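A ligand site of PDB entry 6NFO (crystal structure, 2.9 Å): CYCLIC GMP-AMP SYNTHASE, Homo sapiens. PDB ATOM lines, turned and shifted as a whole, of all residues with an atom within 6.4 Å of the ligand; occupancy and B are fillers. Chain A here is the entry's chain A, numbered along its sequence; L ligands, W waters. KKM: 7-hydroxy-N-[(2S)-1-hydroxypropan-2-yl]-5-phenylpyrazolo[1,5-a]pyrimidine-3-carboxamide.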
ATOM      1  N   MET A  69       2.752  -5.286   4.843  1.00  0.00           N
ATOM      2  CA  MET A  69       2.495  -5.857   3.519  1.00  0.00           C
ATOM      3  C   MET A  69       1.490  -7.000   3.581  1.00  0.00           C
ATOM      4  O   MET A  69       1.598  -7.890   4.416  1.00  0.00           O
ATOM      5  CB  MET A  69       3.787  -6.319   2.864  1.00  0.00           C
ATOM      6  CG  MET A  69       4.407  -5.290   1.983  1.00  0.00           C
ATOM      7  SD  MET A  69       4.295  -5.804   0.262  1.00  0.00           S
ATOM      8  CE  MET A  69       6.069  -5.639  -0.233  1.00  0.00           C
ATOM      9  N   ALA A  87       9.854  -2.379 -15.283  1.00  0.00           N
ATOM     10  CA  ALA A  87       9.482  -2.462 -13.860  1.00  0.00           C
ATOM     11  C   ALA A  87       7.986  -2.398 -13.672  1.00  0.00           C
ATOM     12  O   ALA A  87       7.469  -2.892 -12.663  1.00  0.00           O
ATOM     13  CB  ALA A  87      10.153  -1.402 -13.005  1.00  0.00           C
ATOM     14  N   TYR A  88       7.286  -1.772 -14.634  1.00  0.00           N
ATOM     15  CA  TYR A  88       5.834  -1.609 -14.609  1.00  0.00           C
ATOM     16  C   TYR A  88       5.179  -2.551 -15.596  1.00  0.00           C
ATOM     17  O   TYR A  88       5.682  -2.750 -16.701  1.00  0.00           O
ATOM     18  CB  TYR A  88       5.432  -0.144 -14.850  1.00  0.00           C
ATOM     19  CG  TYR A  88       6.013   0.779 -13.801  1.00  0.00           C
ATOM     20  CD1 TYR A  88       5.407   0.907 -12.552  1.00  0.00           C
ATOM     21  CD2 TYR A  88       7.214   1.443 -14.010  1.00  0.00           C
ATOM     22  CE1 TYR A  88       5.948   1.732 -11.562  1.00  0.00           C
ATOM     23  CE2 TYR A  88       7.754   2.281 -13.038  1.00  0.00           C
ATOM     24  CZ  TYR A  88       7.113   2.435 -11.818  1.00  0.00           C
ATOM     25  OH  TYR A  88       7.659   3.258 -10.869  1.00  0.00           O
ATOM     26  N   LYS A 202       1.410   0.548  -8.507  1.00  0.00           N
ATOM     27  CA  LYS A 202       2.141   1.811  -8.630  1.00  0.00           C
ATOM     28  C   LYS A 202       1.928   2.298 -10.068  1.00  0.00           C
ATOM     29  O   LYS A 202       2.186   1.544 -11.009  1.00  0.00           O
ATOM     30  CB  LYS A 202       3.634   1.593  -8.346  1.00  0.00           C
ATOM     31  CG  LYS A 202       4.451   2.768  -7.847  1.00  0.00           C
ATOM     32  CD  LYS A 202       4.161   3.202  -6.433  1.00  0.00           C
ATOM     33  CE  LYS A 202       5.204   4.129  -5.878  1.00  0.00           C
ATOM     34  NZ  LYS A 202       4.672   4.995  -4.796  1.00  0.00           N
ATOM     35  N   ALA A 204       3.501   4.896 -11.442  1.00  0.00           N
ATOM     36  CA  ALA A 204       4.748   5.574 -11.798  1.00  0.00           C
ATOM     37  C   ALA A 204       5.482   4.984 -13.013  1.00  0.00           C
ATOM     38  O   ALA A 204       5.136   5.266 -14.170  1.00  0.00           O
ATOM     39  CB  ALA A 204       5.664   5.634 -10.594  1.00  0.00           C
ATOM     40  N   ARG A 216       4.021  -2.493 -10.150  1.00  0.00           N
ATOM     41  CA  ARG A 216       5.479  -2.520 -10.091  1.00  0.00           C
ATOM     42  C   ARG A 216       5.967  -3.767  -9.380  1.00  0.00           C
ATOM     43  O   ARG A 216       5.339  -4.210  -8.432  1.00  0.00           O
ATOM     44  CB  ARG A 216       6.021  -1.249  -9.413  1.00  0.00           C
ATOM     45  CG  ARG A 216       7.530  -1.064  -9.558  1.00  0.00           C
ATOM     46  CD  ARG A 216       8.022   0.221  -8.932  1.00  0.00           C
ATOM     47  NE  ARG A 216       7.777   0.275  -7.487  1.00  0.00           N
ATOM     48  CZ  ARG A 216       7.784   1.389  -6.772  1.00  0.00           C
ATOM     49  NH1 ARG A 216       8.030   2.563  -7.361  1.00  0.00           N
ATOM     50  NH2 ARG A 216       7.546   1.362  -5.472  1.00  0.00           N
ATOM     51  N   LEU A 217       7.099  -4.304  -9.836  1.00  0.00           N
ATOM     52  CA  LEU A 217       7.732  -5.491  -9.258  1.00  0.00           C
ATOM     53  C   LEU A 217       8.277  -5.218  -7.852  1.00  0.00           C
ATOM     54  O   LEU A 217       8.837  -4.142  -7.601  1.00  0.00           O
ATOM     55  CB  LEU A 217       8.877  -5.958 -10.158  1.00  0.00           C
ATOM     56  CG  LEU A 217       8.476  -6.567 -11.498  1.00  0.00           C
ATOM     57  CD1 LEU A 217       9.662  -6.632 -12.420  1.00  0.00           C
ATOM     58  CD2 LEU A 217       7.909  -7.932 -11.300  1.00  0.00           C
ATOM     59  N   SER A 218       8.119  -6.193  -6.949  1.00  0.00           N
ATOM     60  CA  SER A 218       8.619  -6.085  -5.583  1.00  0.00           C
ATOM     61  C   SER A 218       9.389  -7.351  -5.201  1.00  0.00           C
ATOM     62  O   SER A 218       8.962  -8.463  -5.520  1.00  0.00           O
ATOM     63  CB  SER A 218       7.495  -5.771  -4.595  1.00  0.00           C
ATOM     64  OG  SER A 218       7.972  -5.557  -3.275  1.00  0.00           O
ATOM     65  N   PHE A 219      10.570  -7.175  -4.559  1.00  0.00           N
ATOM     66  CA  PHE A 219      11.448  -8.254  -4.097  1.00  0.00           C
ATOM     67  C   PHE A 219      11.905  -7.981  -2.646  1.00  0.00           C
ATOM     68  O   PHE A 219      13.037  -8.279  -2.300  1.00  0.00           O
ATOM     69  CB  PHE A 219      12.652  -8.459  -5.031  1.00  0.00           C
ATOM     70  CG  PHE A 219      12.291  -8.704  -6.480  1.00  0.00           C
ATOM     71  CD1 PHE A 219      11.884  -9.964  -6.903  1.00  0.00           C
ATOM     72  CD2 PHE A 219      12.369  -7.683  -7.422  1.00  0.00           C
ATOM     73  CE1 PHE A 219      11.549 -10.199  -8.237  1.00  0.00           C
ATOM     74  CE2 PHE A 219      12.047  -7.923  -8.766  1.00  0.00           C
ATOM     75  CZ  PHE A 219      11.635  -9.177  -9.167  1.00  0.00           C
ATOM     76  N   SER A 220      10.989  -7.407  -1.813  1.00  0.00           N
ATOM     77  CA  SER A 220      11.203  -7.104  -0.395  1.00  0.00           C
ATOM     78  C   SER A 220      11.610  -8.352   0.381  1.00  0.00           C
ATOM     79  O   SER A 220      12.424  -8.246   1.290  1.00  0.00           O
ATOM     80  CB  SER A 220       9.941  -6.501   0.215  1.00  0.00           C
ATOM     81  OG  SER A 220       8.838  -7.393   0.098  1.00  0.00           O
ATOM     82  N   GLU A 223      15.275  -9.158  -0.376  1.00  0.00           N
ATOM     83  CA  GLU A 223      16.071  -8.142   0.309  1.00  0.00           C
ATOM     84  C   GLU A 223      16.258  -8.517   1.794  1.00  0.00           C
ATOM     85  O   GLU A 223      17.358  -8.351   2.348  1.00  0.00           O
ATOM     86  CB  GLU A 223      15.408  -6.754   0.158  1.00  0.00           C
ATOM     87  CG  GLU A 223      15.516  -6.161  -1.240  1.00  0.00           C
ATOM     88  CD  GLU A 223      14.540  -5.058  -1.623  1.00  0.00           C
ATOM     89  OE1 GLU A 223      13.788  -4.571  -0.742  1.00  0.00           O
ATOM     90  OE2 GLU A 223      14.509  -4.691  -2.824  1.00  0.00           O
ATOM     91  N   LYS A 272      11.913  13.688  -3.189  1.00  0.00           N
ATOM     92  CA  LYS A 272      11.995  12.583  -4.151  1.00  0.00           C
ATOM     93  C   LYS A 272      12.959  11.397  -3.731  1.00  0.00           C
ATOM     94  O   LYS A 272      12.889  10.296  -4.296  1.00  0.00           O
ATOM     95  CB  LYS A 272      12.320  13.113  -5.563  1.00  0.00           C
ATOM     96  N   PHE A 273      13.805  11.615  -2.729  1.00  0.00           N
ATOM     97  CA  PHE A 273      14.716  10.565  -2.260  1.00  0.00           C
ATOM     98  C   PHE A 273      14.056   9.688  -1.204  1.00  0.00           C
ATOM     99  O   PHE A 273      13.298  10.182  -0.383  1.00  0.00           O
ATOM    100  CB  PHE A 273      16.027  11.163  -1.741  1.00  0.00           C
ATOM    101  CG  PHE A 273      16.755  11.944  -2.798  1.00  0.00           C
ATOM    102  CD1 PHE A 273      17.534  11.308  -3.754  1.00  0.00           C
ATOM    103  CD2 PHE A 273      16.663  13.330  -2.838  1.00  0.00           C
ATOM    104  CE1 PHE A 273      18.212  12.040  -4.721  1.00  0.00           C
ATOM    105  CE2 PHE A 273      17.362  14.058  -3.804  1.00  0.00           C
ATOM    106  CZ  PHE A 273      18.123  13.402  -4.733  1.00  0.00           C
ATOM    107  N   SER A 274      14.350   8.388  -1.218  1.00  0.00           N
ATOM    108  CA  SER A 274      13.797   7.459  -0.244  1.00  0.00           C
ATOM    109  C   SER A 274      14.869   6.517   0.296  1.00  0.00           C
ATOM    110  O   SER A 274      15.962   6.390  -0.308  1.00  0.00           O
ATOM    111  CB  SER A 274      12.641   6.666  -0.855  1.00  0.00           C
ATOM    112  OG  SER A 274      13.071   5.486  -1.500  1.00  0.00           O
ATOM    113  N   SER A 275      14.538   5.789   1.400  1.00  0.00           N
ATOM    114  CA  SER A 275      15.468   4.825   1.966  1.00  0.00           C
ATOM    115  C   SER A 275      15.768   3.706   0.947  1.00  0.00           C
ATOM    116  O   SER A 275      16.814   3.051   1.055  1.00  0.00           O
ATOM    117  CB  SER A 275      14.946   4.254   3.277  1.00  0.00           C
ATOM    118  OG  SER A 275      13.836   3.396   3.054  1.00  0.00           O
ATOM    119  N   TYR A 276      14.890   3.532  -0.060  1.00  0.00           N
ATOM    120  CA  TYR A 276      15.110   2.529  -1.096  1.00  0.00           C
ATOM    121  C   TYR A 276      16.321   2.850  -1.952  1.00  0.00           C
ATOM    122  O   TYR A 276      17.018   1.932  -2.360  1.00  0.00           O
ATOM    123  CB  TYR A 276      13.861   2.269  -1.940  1.00  0.00           C
ATOM    124  CG  TYR A 276      14.010   0.989  -2.723  1.00  0.00           C
ATOM    125  CD1 TYR A 276      13.995  -0.253  -2.088  1.00  0.00           C
ATOM    126  CD2 TYR A 276      14.258   1.008  -4.095  1.00  0.00           C
ATOM    127  CE1 TYR A 276      14.162  -1.433  -2.802  1.00  0.00           C
ATOM    128  CE2 TYR A 276      14.448  -0.175  -4.818  1.00  0.00           C
ATOM    129  CZ  TYR A 276      14.404  -1.396  -4.161  1.00  0.00           C
ATOM    130  OH  TYR A 276      14.589  -2.590  -4.825  1.00  0.00           O
ATOM    131  N   HIS A 277      16.596   4.146  -2.173  1.00  0.00           N
ATOM    132  CA  HIS A 277      17.777   4.580  -2.930  1.00  0.00           C
ATOM    133  C   HIS A 277      19.047   4.208  -2.170  1.00  0.00           C
ATOM    134  O   HIS A 277      20.006   3.714  -2.753  1.00  0.00           O
ATOM    135  CB  HIS A 277      17.724   6.103  -3.177  1.00  0.00           C
ATOM    136  CG  HIS A 277      16.592   6.551  -4.047  1.00  0.00           C
ATOM    137  ND1 HIS A 277      15.688   7.491  -3.609  1.00  0.00           N
ATOM    138  CD2 HIS A 277      16.255   6.165  -5.285  1.00  0.00           C
ATOM    139  CE1 HIS A 277      14.834   7.646  -4.590  1.00  0.00           C
ATOM    140  NE2 HIS A 277      15.120   6.859  -5.616  1.00  0.00           N
ATOM    141  N   LYS A 279      19.303   1.780   0.278  1.00  0.00           N
ATOM    142  CA  LYS A 279      19.336   0.330   0.353  1.00  0.00           C
ATOM    143  C   LYS A 279      19.888  -0.277  -0.959  1.00  0.00           C
ATOM    144  O   LYS A 279      20.715  -1.187  -0.889  1.00  0.00           O
ATOM    145  CB  LYS A 279      17.912  -0.155   0.628  1.00  0.00           C
ATOM    146  CG  LYS A 279      17.818  -1.600   1.070  1.00  0.00           C
ATOM    147  CD  LYS A 279      16.510  -1.812   1.785  1.00  0.00           C
ATOM    148  CE  LYS A 279      15.631  -2.757   1.025  1.00  0.00           C
ATOM    149  NZ  LYS A 279      14.955  -3.713   1.945  1.00  0.00           N
ATOM    150  N   ASN A 322      18.295  -0.333 -10.342  1.00  0.00           N
ATOM    151  CA  ASN A 322      17.556  -1.229  -9.457  1.00  0.00           C
ATOM    152  C   ASN A 322      18.372  -2.545  -9.354  1.00  0.00           C
ATOM    153  O   ASN A 322      18.823  -3.085 -10.388  1.00  0.00           O
ATOM    154  CB  ASN A 322      16.156  -1.508 -10.031  1.00  0.00           C
ATOM    155  CG  ASN A 322      15.309  -2.392  -9.142  1.00  0.00           C
ATOM    156  OD1 ASN A 322      15.461  -3.616  -9.092  1.00  0.00           O
ATOM    157  ND2 ASN A 322      14.434  -1.787  -8.371  1.00  0.00           N
ATOM    158  N   ILE A 325      16.370  -5.187 -11.363  1.00  0.00           N
ATOM    159  CA  ILE A 325      16.058  -4.750 -12.725  1.00  0.00           C
ATOM    160  C   ILE A 325      17.179  -3.787 -13.195  1.00  0.00           C
ATOM    161  O   ILE A 325      17.077  -2.570 -13.029  1.00  0.00           O
ATOM    162  CB  ILE A 325      14.630  -4.126 -12.784  1.00  0.00           C
ATOM    163  CG1 ILE A 325      13.593  -5.102 -12.208  1.00  0.00           C
ATOM    164  CG2 ILE A 325      14.245  -3.743 -14.201  1.00  0.00           C
ATOM    165  CD1 ILE A 325      12.540  -4.486 -11.357  1.00  0.00           C
ATOM    166  N   PHE A 328      16.422  -0.515 -15.131  1.00  0.00           N
ATOM    167  CA  PHE A 328      15.662   0.526 -14.463  1.00  0.00           C
ATOM    168  C   PHE A 328      16.591   1.412 -13.638  1.00  0.00           C
ATOM    169  O   PHE A 328      17.176   0.941 -12.669  1.00  0.00           O
ATOM    170  CB  PHE A 328      14.491  -0.024 -13.612  1.00  0.00           C
ATOM    171  CG  PHE A 328      13.504   1.059 -13.237  1.00  0.00           C
ATOM    172  CD1 PHE A 328      13.761   1.897 -12.164  1.00  0.00           C
ATOM    173  CD2 PHE A 328      12.375   1.293 -14.001  1.00  0.00           C
ATOM    174  CE1 PHE A 328      12.877   2.934 -11.851  1.00  0.00           C
ATOM    175  CE2 PHE A 328      11.485   2.303 -13.662  1.00  0.00           C
ATOM    176  CZ  PHE A 328      11.748   3.124 -12.601  1.00  0.00           C
ATOM    177  N   LEU A 330      16.802   4.313 -11.054  1.00  0.00           N
ATOM    178  CA  LEU A 330      16.121   5.076  -9.979  1.00  0.00           C
ATOM    179  C   LEU A 330      16.534   6.562  -9.945  1.00  0.00           C
ATOM    180  O   LEU A 330      15.795   7.372  -9.375  1.00  0.00           O
ATOM    181  CB  LEU A 330      16.384   4.450  -8.571  1.00  0.00           C
ATOM    182  CG  LEU A 330      16.283   2.932  -8.364  1.00  0.00           C
ATOM    183  CD1 LEU A 330      16.657   2.559  -6.967  1.00  0.00           C
ATOM    184  CD2 LEU A 330      14.916   2.424  -8.608  1.00  0.00           C
ATOM    185  N   LEU A 335      13.065  11.140 -13.483  1.00  0.00           N
ATOM    186  CA  LEU A 335      12.536  10.826 -12.151  1.00  0.00           C
ATOM    187  C   LEU A 335      12.928  11.832 -11.101  1.00  0.00           C
ATOM    188  O   LEU A 335      12.110  12.190 -10.256  1.00  0.00           O
ATOM    189  CB  LEU A 335      12.989   9.428 -11.692  1.00  0.00           C
ATOM    190  CG  LEU A 335      12.576   8.265 -12.566  1.00  0.00           C
ATOM    191  CD1 LEU A 335      13.173   6.975 -12.068  1.00  0.00           C
ATOM    192  CD2 LEU A 335      11.088   8.165 -12.608  1.00  0.00           C
HETATM  193  C10 KKM L   1      11.021  -1.434  -8.120  1.00  0.00           C
HETATM  194  C13 KKM L   1      10.504   1.602  -2.709  1.00  0.00           C
HETATM  195  C17 KKM L   1      10.017   5.262  -5.984  1.00  0.00           C
HETATM  196  C21 KKM L   1      10.333   1.007  -1.490  1.00  0.00           C
HETATM  197  O01 KKM L   1      10.515  -2.963  -3.045  1.00  0.00           O
HETATM  198  C02 KKM L   1      10.668  -1.749  -3.726  1.00  0.00           C
HETATM  199  C03 KKM L   1      10.832  -1.734  -5.083  1.00  0.00           C
HETATM  200  C04 KKM L   1      10.907  -0.515  -5.738  1.00  0.00           C
HETATM  201  C05 KKM L   1      11.145  -0.363  -7.241  1.00  0.00           C
HETATM  202  C06 KKM L   1      11.449   0.910  -7.748  1.00  0.00           C
HETATM  203  C07 KKM L   1      11.703   1.096  -9.101  1.00  0.00           C
HETATM  204  C08 KKM L   1      11.641   0.020  -9.967  1.00  0.00           C
HETATM  205  C09 KKM L   1      11.270  -1.227  -9.480  1.00  0.00           C
HETATM  206  N11 KKM L   1      10.848   0.613  -5.025  1.00  0.00           N
HETATM  207  C12 KKM L   1      10.667   0.581  -3.661  1.00  0.00           C
HETATM  208  C14 KKM L   1      10.598   3.097  -2.991  1.00  0.00           C
HETATM  209  N15 KKM L   1      10.648   3.586  -4.359  1.00  0.00           N
HETATM  210  C16 KKM L   1      10.760   4.985  -4.666  1.00  0.00           C
HETATM  211  O18 KKM L   1      10.719   4.753  -7.097  1.00  0.00           O
HETATM  212  C19 KKM L   1      12.257   5.360  -4.700  1.00  0.00           C
HETATM  213  O20 KKM L   1      10.635   3.855  -2.079  1.00  0.00           O
HETATM  214  N23 KKM L   1      10.614  -0.597  -3.029  1.00  0.00           N
HETATM  215  N22 KKM L   1      10.387  -0.366  -1.685  1.00  0.00           N
HETATM  216  O   HOH W   1      11.990  -4.777  -4.432  1.00  0.00           O
HETATM  217  O   HOH W   2      13.069  -3.986  -7.099  1.00  0.00           O
HETATM  218  O   HOH W   3       7.773  -2.043  -6.005  1.00  0.00           O
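The guanidinium group (NH2) of Arg 216 sits at hydrogen-bond distance from a nitrogen (N11) of the ligand, at 3.4 Å. The side-chain hydroxyl of Ser 274 sits at hydrogen-bond distance from an oxygen (O20) of the ligand, 3.0 Å away.
N of Asn 322 is in hydrogen-bond range of O of Phe 328 (2.9 Å). N of Tyr 276 lies close to OG of Ser 274, 3.0 Å away. OE2 of Glu 223 is in hydrogen-bond range of OH of Tyr 276, at 2.9 Å. N of Ile 325 is in hydrogen-bond range of OD1 of Asn 322. The backbone NH (N) of Leu 217 sits at hydrogen-bond distance from the backbone carbonyl oxygen (O) of Ala 87. A ring nitrogen (ND1) of His 277 is in hydrogen-bond range of the backbone NH of Ser 274 (2.9 Å).
Ala 87 touches the ligand. O of Leu 217 touches C10 of the ligand (3.5 Å). OG of Ser 218 touches O01 of the ligand, 3.6 Å away. Tyr 276 touches the ligand (CG to C12, 3.5 Å). His 277 touches the ligand. Asn 322 touches the ligand. CD1 of Ile 325 touches C09 of the ligand, 3.97 Å away. Phe 328 touches the ligand. Leu 330 touches the ligand (CD2 to C07, 3.5 Å). Hydrophobic or aromatic side chains that line the ligand: Ala 87, Tyr 276, His 277, Ile 325, Phe 328 and Leu 330.
Water W1 lies within hydrogen-bond range of an oxygen (O01) of the ligand (2.7 Å), the backbone NH (N) of Phe 219 (2.8 Å), the side-chain carboxylate (OE2) of Glu 223 (3.0 Å) and the side-chain hydroxyl (OH) of Tyr 276 (3.4 Å). Water W3 bridges NE of Arg 216 (2.8 Å) and O of Leu 217 (2.8 Å). Water W2 lies within hydrogen-bond range of the side-chain amide nitrogen of Asn 322 (2.9 Å) and the side-chain hydroxyl of Tyr 276 (3.1 Å).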
